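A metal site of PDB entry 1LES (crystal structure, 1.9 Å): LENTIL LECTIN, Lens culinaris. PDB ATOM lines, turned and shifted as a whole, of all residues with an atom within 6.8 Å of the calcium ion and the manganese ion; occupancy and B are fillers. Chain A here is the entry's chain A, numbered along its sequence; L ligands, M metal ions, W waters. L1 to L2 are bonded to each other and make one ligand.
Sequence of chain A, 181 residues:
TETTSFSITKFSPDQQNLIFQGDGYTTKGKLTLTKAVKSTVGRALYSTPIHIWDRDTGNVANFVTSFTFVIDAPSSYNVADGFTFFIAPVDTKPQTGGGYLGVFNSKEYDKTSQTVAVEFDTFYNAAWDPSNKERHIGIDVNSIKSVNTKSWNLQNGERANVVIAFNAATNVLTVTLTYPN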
ATOM      1  N   ASP A  81       2.701   5.407  17.519  1.00  0.00           N
ATOM      2  CA  ASP A  81       3.006   4.018  17.165  1.00  0.00           C
ATOM      3  C   ASP A  81       3.113   3.097  18.368  1.00  0.00           C
ATOM      4  O   ASP A  81       3.004   1.877  18.232  1.00  0.00           O
ATOM      5  CB  ASP A  81       4.303   3.959  16.385  1.00  0.00           C
ATOM      6  CG  ASP A  81       4.062   3.992  14.888  1.00  0.00           C
ATOM      7  OD1 ASP A  81       3.685   2.931  14.304  1.00  0.00           O
ATOM      8  OD2 ASP A  81       4.247   5.068  14.312  1.00  0.00           O
ATOM      9  N   GLY A  98       8.799   5.645  13.846  1.00  0.00           N
ATOM     10  CA  GLY A  98       7.609   4.997  13.300  1.00  0.00           C
ATOM     11  C   GLY A  98       7.327   3.635  13.918  1.00  0.00           C
ATOM     12  O   GLY A  98       7.510   3.445  15.135  1.00  0.00           O
ATOM     13  N   GLY A  99       6.968   2.649  13.125  1.00  0.00           N
ATOM     14  CA  GLY A  99       6.651   1.377  13.721  1.00  0.00           C
ATOM     15  C   GLY A  99       7.891   0.686  14.322  1.00  0.00           C
ATOM     16  O   GLY A  99       7.740  -0.371  14.931  1.00  0.00           O
ATOM     17  N   TYR A 100       9.099   1.196  14.114  1.00  0.00           N
ATOM     18  CA  TYR A 100      10.257   0.527  14.715  1.00  0.00           C
ATOM     19  C   TYR A 100      10.486   0.953  16.159  1.00  0.00           C
ATOM     20  O   TYR A 100      11.428   0.519  16.820  1.00  0.00           O
ATOM     21  CB  TYR A 100      11.507   0.736  13.896  1.00  0.00           C
ATOM     22  CG  TYR A 100      11.460  -0.030  12.625  1.00  0.00           C
ATOM     23  CD1 TYR A 100      11.914  -1.331  12.549  1.00  0.00           C
ATOM     24  CD2 TYR A 100      10.954   0.571  11.487  1.00  0.00           C
ATOM     25  CE1 TYR A 100      11.871  -2.026  11.354  1.00  0.00           C
ATOM     26  CE2 TYR A 100      10.902  -0.103  10.283  1.00  0.00           C
ATOM     27  CZ  TYR A 100      11.361  -1.384  10.228  1.00  0.00           C
ATOM     28  OH  TYR A 100      11.268  -1.993   9.016  1.00  0.00           O
ATOM     29  N   LEU A 101       9.632   1.838  16.619  1.00  0.00           N
ATOM     30  CA  LEU A 101       9.609   2.280  17.986  1.00  0.00           C
ATOM     31  C   LEU A 101      10.891   2.946  18.527  1.00  0.00           C
ATOM     32  O   LEU A 101      11.017   3.095  19.752  1.00  0.00           O
ATOM     33  CB  LEU A 101       9.138   1.112  18.875  1.00  0.00           C
ATOM     34  CG  LEU A 101       7.743   0.544  18.498  1.00  0.00           C
ATOM     35  CD1 LEU A 101       7.392  -0.668  19.314  1.00  0.00           C
ATOM     36  CD2 LEU A 101       6.699   1.575  18.687  1.00  0.00           C
ATOM     37  N   GLU A 119       7.248  -4.007  24.299  1.00  0.00           N
ATOM     38  CA  GLU A 119       6.450  -2.997  23.581  1.00  0.00           C
ATOM     39  C   GLU A 119       4.972  -2.924  23.899  1.00  0.00           C
ATOM     40  O   GLU A 119       4.366  -3.900  24.317  1.00  0.00           O
ATOM     41  CB  GLU A 119       6.620  -3.154  22.080  1.00  0.00           C
ATOM     42  CG  GLU A 119       6.219  -4.501  21.623  1.00  0.00           C
ATOM     43  CD  GLU A 119       6.153  -4.611  20.115  1.00  0.00           C
ATOM     44  OE1 GLU A 119       7.149  -4.370  19.391  1.00  0.00           O
ATOM     45  OE2 GLU A 119       5.054  -5.001  19.650  1.00  0.00           O
ATOM     46  N   ASP A 121       2.408  -1.758  21.686  1.00  0.00           N
ATOM     47  CA  ASP A 121       2.251  -1.382  20.278  1.00  0.00           C
ATOM     48  C   ASP A 121       0.790  -1.009  19.938  1.00  0.00           C
ATOM     49  O   ASP A 121      -0.123  -1.841  20.022  1.00  0.00           O
ATOM     50  CB  ASP A 121       2.741  -2.589  19.464  1.00  0.00           C
ATOM     51  CG  ASP A 121       2.888  -2.309  17.976  1.00  0.00           C
ATOM     52  OD1 ASP A 121       2.355  -1.296  17.474  1.00  0.00           O
ATOM     53  OD2 ASP A 121       3.595  -3.110  17.331  1.00  0.00           O
ATOM     54  N   THR A 122       0.562   0.214  19.489  1.00  0.00           N
ATOM     55  CA  THR A 122      -0.789   0.646  19.210  1.00  0.00           C
ATOM     56  C   THR A 122      -1.192   0.671  17.705  1.00  0.00           C
ATOM     57  O   THR A 122      -2.314   1.052  17.397  1.00  0.00           O
ATOM     58  CB  THR A 122      -0.980   2.049  19.723  1.00  0.00           C
ATOM     59  OG1 THR A 122       0.050   2.860  19.171  1.00  0.00           O
ATOM     60  CG2 THR A 122      -0.981   2.096  21.277  1.00  0.00           C
ATOM     61  N   PHE A 123      -0.291   0.279  16.784  1.00  0.00           N
ATOM     62  CA  PHE A 123      -0.573   0.372  15.342  1.00  0.00           C
ATOM     63  C   PHE A 123      -0.145  -0.846  14.588  1.00  0.00           C
ATOM     64  O   PHE A 123       0.987  -1.327  14.745  1.00  0.00           O
ATOM     65  CB  PHE A 123       0.119   1.599  14.759  1.00  0.00           C
ATOM     66  CG  PHE A 123      -0.104   1.780  13.292  1.00  0.00           C
ATOM     67  CD1 PHE A 123       0.759   1.157  12.350  1.00  0.00           C
ATOM     68  CD2 PHE A 123      -1.182   2.553  12.829  1.00  0.00           C
ATOM     69  CE1 PHE A 123       0.565   1.281  10.969  1.00  0.00           C
ATOM     70  CE2 PHE A 123      -1.386   2.695  11.456  1.00  0.00           C
ATOM     71  CZ  PHE A 123      -0.493   2.049  10.528  1.00  0.00           C
ATOM     72  N   TYR A 124      -1.050  -1.352  13.736  1.00  0.00           N
ATOM     73  CA  TYR A 124      -0.748  -2.580  13.011  1.00  0.00           C
ATOM     74  C   TYR A 124       0.133  -2.404  11.838  1.00  0.00           C
ATOM     75  O   TYR A 124      -0.268  -1.743  10.878  1.00  0.00           O
ATOM     76  CB  TYR A 124      -2.050  -3.269  12.576  1.00  0.00           C
ATOM     77  CG  TYR A 124      -1.848  -4.425  11.595  1.00  0.00           C
ATOM     78  CD1 TYR A 124      -1.257  -5.607  11.996  1.00  0.00           C
ATOM     79  CD2 TYR A 124      -2.281  -4.325  10.271  1.00  0.00           C
ATOM     80  CE1 TYR A 124      -1.095  -6.668  11.093  1.00  0.00           C
ATOM     81  CE2 TYR A 124      -2.115  -5.372   9.377  1.00  0.00           C
ATOM     82  CZ  TYR A 124      -1.533  -6.530   9.799  1.00  0.00           C
ATOM     83  OH  TYR A 124      -1.313  -7.566   8.932  1.00  0.00           O
ATOM     84  N   ASN A 125       1.380  -2.891  11.905  1.00  0.00           N
ATOM     85  CA  ASN A 125       2.344  -2.818  10.777  1.00  0.00           C
ATOM     86  C   ASN A 125       2.270  -4.199  10.123  1.00  0.00           C
ATOM     87  O   ASN A 125       2.777  -5.199  10.638  1.00  0.00           O
ATOM     88  CB  ASN A 125       3.802  -2.510  11.219  1.00  0.00           C
ATOM     89  CG  ASN A 125       3.931  -1.174  11.926  1.00  0.00           C
ATOM     90  OD1 ASN A 125       3.765  -1.079  13.166  1.00  0.00           O
ATOM     91  ND2 ASN A 125       4.122  -0.100  11.140  1.00  0.00           N
ATOM     92  N   TRP A 128       4.967  -7.142   9.925  1.00  0.00           N
ATOM     93  CA  TRP A 128       5.452  -7.989  11.039  1.00  0.00           C
ATOM     94  C   TRP A 128       4.528  -8.135  12.226  1.00  0.00           C
ATOM     95  O   TRP A 128       4.725  -9.039  13.050  1.00  0.00           O
ATOM     96  CB  TRP A 128       6.840  -7.503  11.595  1.00  0.00           C
ATOM     97  CG  TRP A 128       6.833  -6.014  12.124  1.00  0.00           C
ATOM     98  CD1 TRP A 128       6.258  -5.556  13.302  1.00  0.00           C
ATOM     99  CD2 TRP A 128       7.322  -4.837  11.448  1.00  0.00           C
ATOM    100  NE1 TRP A 128       6.336  -4.177  13.353  1.00  0.00           N
ATOM    101  CE2 TRP A 128       6.992  -3.717  12.243  1.00  0.00           C
ATOM    102  CE3 TRP A 128       8.009  -4.620  10.234  1.00  0.00           C
ATOM    103  CZ2 TRP A 128       7.319  -2.412  11.881  1.00  0.00           C
ATOM    104  CZ3 TRP A 128       8.338  -3.309   9.885  1.00  0.00           C
ATOM    105  CH2 TRP A 128       7.988  -2.236  10.712  1.00  0.00           C
ATOM    106  N   ASP A 129       3.575  -7.232  12.392  1.00  0.00           N
ATOM    107  CA  ASP A 129       2.713  -7.334  13.560  1.00  0.00           C
ATOM    108  C   ASP A 129       1.745  -8.508  13.503  1.00  0.00           C
ATOM    109  O   ASP A 129       1.433  -9.006  12.424  1.00  0.00           O
ATOM    110  CB  ASP A 129       2.000  -6.017  13.740  1.00  0.00           C
ATOM    111  CG  ASP A 129       2.847  -5.007  14.492  1.00  0.00           C
ATOM    112  OD1 ASP A 129       3.704  -5.490  15.264  1.00  0.00           O
ATOM    113  OD2 ASP A 129       2.656  -3.785  14.359  1.00  0.00           O
ATOM    114  N   PRO A 130       1.272  -8.997  14.651  1.00  0.00           N
ATOM    115  CA  PRO A 130       0.343 -10.137  14.637  1.00  0.00           C
ATOM    116  C   PRO A 130      -0.905  -9.917  13.752  1.00  0.00           C
ATOM    117  O   PRO A 130      -1.565  -8.867  13.837  1.00  0.00           O
ATOM    118  CB  PRO A 130       0.028 -10.360  16.128  1.00  0.00           C
ATOM    119  CG  PRO A 130       0.322  -9.034  16.764  1.00  0.00           C
ATOM    120  CD  PRO A 130       1.514  -8.519  16.023  1.00  0.00           C
ATOM    121  N   HIS A 136      -1.278  -4.609  20.952  1.00  0.00           N
ATOM    122  CA  HIS A 136      -0.724  -5.688  21.725  1.00  0.00           C
ATOM    123  C   HIS A 136       0.512  -5.313  22.533  1.00  0.00           C
ATOM    124  O   HIS A 136       1.239  -4.375  22.196  1.00  0.00           O
ATOM    125  CB  HIS A 136      -0.276  -6.797  20.738  1.00  0.00           C
ATOM    126  CG  HIS A 136       0.623  -6.308  19.630  1.00  0.00           C
ATOM    127  ND1 HIS A 136       0.143  -5.637  18.511  1.00  0.00           N
ATOM    128  CD2 HIS A 136       1.962  -6.384  19.465  1.00  0.00           C
ATOM    129  CE1 HIS A 136       1.152  -5.343  17.715  1.00  0.00           C
ATOM    130  NE2 HIS A 136       2.274  -5.784  18.270  1.00  0.00           N
ATOM    131  N   ILE A 137       0.789  -6.169  23.520  1.00  0.00           N
ATOM    132  CA  ILE A 137       1.977  -6.090  24.375  1.00  0.00           C
ATOM    133  C   ILE A 137       2.889  -7.166  23.769  1.00  0.00           C
ATOM    134  O   ILE A 137       2.430  -8.238  23.444  1.00  0.00           O
ATOM    135  CB  ILE A 137       1.646  -6.512  25.780  1.00  0.00           C
ATOM    136  CG1 ILE A 137       0.663  -5.535  26.379  1.00  0.00           C
ATOM    137  CG2 ILE A 137       2.933  -6.583  26.591  1.00  0.00           C
ATOM    138  CD1 ILE A 137       0.087  -6.056  27.688  1.00  0.00           C
ATOM    139  N   GLY A 138       4.188  -6.923  23.625  1.00  0.00           N
ATOM    140  CA  GLY A 138       5.039  -7.929  23.034  1.00  0.00           C
ATOM    141  C   GLY A 138       6.443  -7.884  23.635  1.00  0.00           C
ATOM    142  O   GLY A 138       6.818  -6.862  24.229  1.00  0.00           O
ATOM    143  N   ASP A 140      10.237  -8.149  22.642  1.00  0.00           N
ATOM    144  CA  ASP A 140      11.082  -8.079  21.468  1.00  0.00           C
ATOM    145  C   ASP A 140      12.556  -8.378  21.827  1.00  0.00           C
ATOM    146  O   ASP A 140      13.090  -7.727  22.705  1.00  0.00           O
ATOM    147  CB  ASP A 140      11.081  -6.658  20.914  1.00  0.00           C
ATOM    148  CG  ASP A 140       9.707  -6.174  20.496  1.00  0.00           C
ATOM    149  OD1 ASP A 140       8.790  -6.990  20.377  1.00  0.00           O
ATOM    150  OD2 ASP A 140       9.546  -4.976  20.285  1.00  0.00           O
ATOM    151  N   ILE A 144      12.090  -6.113  15.690  1.00  0.00           N
ATOM    152  CA  ILE A 144      10.759  -5.478  15.949  1.00  0.00           C
ATOM    153  C   ILE A 144       9.620  -6.525  15.872  1.00  0.00           C
ATOM    154  O   ILE A 144       8.477  -6.294  16.293  1.00  0.00           O
ATOM    155  CB  ILE A 144      10.498  -4.286  14.978  1.00  0.00           C
ATOM    156  CG1 ILE A 144       9.289  -3.469  15.436  1.00  0.00           C
ATOM    157  CG2 ILE A 144      10.353  -4.808  13.544  1.00  0.00           C
ATOM    158  CD1 ILE A 144       9.461  -2.814  16.828  1.00  0.00           C
ATOM    159  N   LYS A 145       9.963  -7.713  15.389  1.00  0.00           N
ATOM    160  CA  LYS A 145       8.973  -8.809  15.314  1.00  0.00           C
ATOM    161  C   LYS A 145       8.977  -9.541  16.639  1.00  0.00           C
ATOM    162  O   LYS A 145       9.856 -10.373  16.834  1.00  0.00           O
ATOM    163  CB  LYS A 145       9.421  -9.778  14.239  1.00  0.00           C
ATOM    164  CG  LYS A 145       8.319 -10.173  13.369  1.00  0.00           C
ATOM    165  CD  LYS A 145       7.907 -11.547  13.640  1.00  0.00           C
ATOM    166  CE  LYS A 145       8.391 -12.439  12.509  1.00  0.00           C
ATOM    167  NZ  LYS A 145       8.111 -13.869  12.899  1.00  0.00           N
ATOM    168  N   SER A 146       8.029  -9.298  17.533  1.00  0.00           N
ATOM    169  CA  SER A 146       8.031  -9.955  18.847  1.00  0.00           C
ATOM    170  C   SER A 146       8.139 -11.461  18.894  1.00  0.00           C
ATOM    171  O   SER A 146       7.654 -12.149  18.011  1.00  0.00           O
ATOM    172  CB  SER A 146       6.775  -9.576  19.600  1.00  0.00           C
ATOM    173  OG  SER A 146       6.544  -8.198  19.440  1.00  0.00           O
ATOM    174  N   THR A 149       3.322 -12.295  21.919  1.00  0.00           N
ATOM    175  CA  THR A 149       2.496 -11.073  22.032  1.00  0.00           C
ATOM    176  C   THR A 149       1.222 -11.373  22.770  1.00  0.00           C
ATOM    177  O   THR A 149       0.867 -12.501  22.897  1.00  0.00           O
ATOM    178  CB  THR A 149       2.044 -10.570  20.657  1.00  0.00           C
ATOM    179  OG1 THR A 149       1.474 -11.662  19.932  1.00  0.00           O
ATOM    180  CG2 THR A 149       3.218 -10.064  19.844  1.00  0.00           C
HETATM  181  C1  LIG L   1       3.842   5.280   8.504  1.00  0.00           C
HETATM  182  C2  LIG L   1       5.244   4.899   9.075  1.00  0.00           C
HETATM  183  C3  LIG L   1       5.169   3.682   9.889  1.00  0.00           C
HETATM  184  C4  LIG L   1       4.264   3.943  11.027  1.00  0.00           C
HETATM  185  C5  LIG L   1       2.808   4.367  10.561  1.00  0.00           C
HETATM  186  C6  LIG L   1       1.896   4.714  11.755  1.00  0.00           C
HETATM  187  O1  LIG L   1       6.094   4.650   8.000  1.00  0.00           O
HETATM  188  O2  LIG L   1       6.505   3.303  10.428  1.00  0.00           O
HETATM  189  O3  LIG L   1       4.194   2.694  11.731  1.00  0.00           O
HETATM  190  O4  LIG L   1       3.047   5.487   9.662  1.00  0.00           O
HETATM  191  O5  LIG L   1       2.291   5.898  12.295  1.00  0.00           O
HETATM  192  C1  LG2 L   2       3.696   4.922   5.387  1.00  0.00           C
HETATM  193  C2  LG2 L   2       2.753   4.375   6.449  1.00  0.00           C
HETATM  194  C3  LG2 L   2       2.161   3.137   5.904  1.00  0.00           C
HETATM  195  C4  LG2 L   2       0.983   3.060   6.865  1.00  0.00           C
HETATM  196  C5  LG2 L   2       0.406   4.397   6.830  1.00  0.00           C
HETATM  197  C6  LG2 L   2      -0.323   4.521   8.111  1.00  0.00           C
HETATM  198  O1  LG2 L   2       2.958   5.393   4.236  1.00  0.00           O
HETATM  199  O2  LG2 L   2       3.379   4.119   7.789  1.00  0.00           O
HETATM  200  O3  LG2 L   2       2.925   2.006   6.196  1.00  0.00           O
HETATM  201  O4  LG2 L   2      -0.027   2.148   6.387  1.00  0.00           O
HETATM  202  O5  LG2 L   2       1.575   5.201   6.664  1.00  0.00           O
HETATM  203  O6  LG2 L   2      -1.010   5.743   8.042  1.00  0.00           O
HETATM  204 CA    CA M   1       3.242  -1.714  15.265  1.00  0.00          CA
HETATM  205 MN    MN M   2       4.211  -5.189  17.437  1.00  0.00          MN
HETATM  206  O   HOH W   1       6.304  -4.561  16.867  1.00  0.00           O
HETATM  207  O   HOH W   2       5.641  -2.135  15.446  1.00  0.00           O
HETATM  208  O   HOH W   3       4.767  -7.103  17.427  1.00  0.00           O
HETATM  209  O   HOH W   4       3.626   0.427  15.789  1.00  0.00           O
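Water W2 lies within hydrogen-bond range of the backbone carbonyl oxygen of Gly 99 and the indole nitrogen of Trp 128. Water W1 bridges OE1 of Glu 119 (2.7 Å) and O of Ile 144 (2.8 Å).
Four residues have an atom within 4 Å of the manganese ion: Glu 119, Asp 121, Asp 129 and His 136. Along chain A the residues within 4 Å of the manganese ion span positions 119 to 136.
The manganese ion is bound by water W3 (2.0 Å), OD2 of Asp 121 (2.2 Å), NE2 of His 136 (2.2 Å), OD1 of Asp 129 (2.3 Å), water W1 (2.3 Å) and OE2 of Glu 119 (2.4 Å).
The calcium ion is bound by water W4 (2.2 Å), the side-chain amide oxygen (OD1) of Asn 125 (2.3 Å), the side-chain carboxylate (OD2) of Asp 129 (2.3 Å), the backbone carbonyl oxygen (O) of Phe 123 (2.3 Å), the side-chain carboxylate (OD1) of Asp 121 (2.4 Å), water W2 (2.4 Å) and the side-chain carboxylate (OD2) of Asp 121 (2.5 Å).
The side-chain carboxylate (OD2) of Asp 140 sits close to the side-chain carboxylate (OE1) of Glu 119 (2.6 Å). The backbone NH (N) of Glu 119 is in hydrogen-bond range of the backbone carbonyl oxygen (O) of Gly 138, at 2.9 Å.
The side-chain amide nitrogen of Asn 125 lies within hydrogen-bond range of an oxygen (O3) of LIG L1 (2.9 Å). The side-chain carboxylate (OD1) of Asp 81 sits at hydrogen-bond distance from an oxygen (O3) of LIG L1 (2.6 Å). The backbone NH (N) of Gly 99 lies within hydrogen-bond range of an oxygen (O2) of LIG L1 (2.8 Å).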
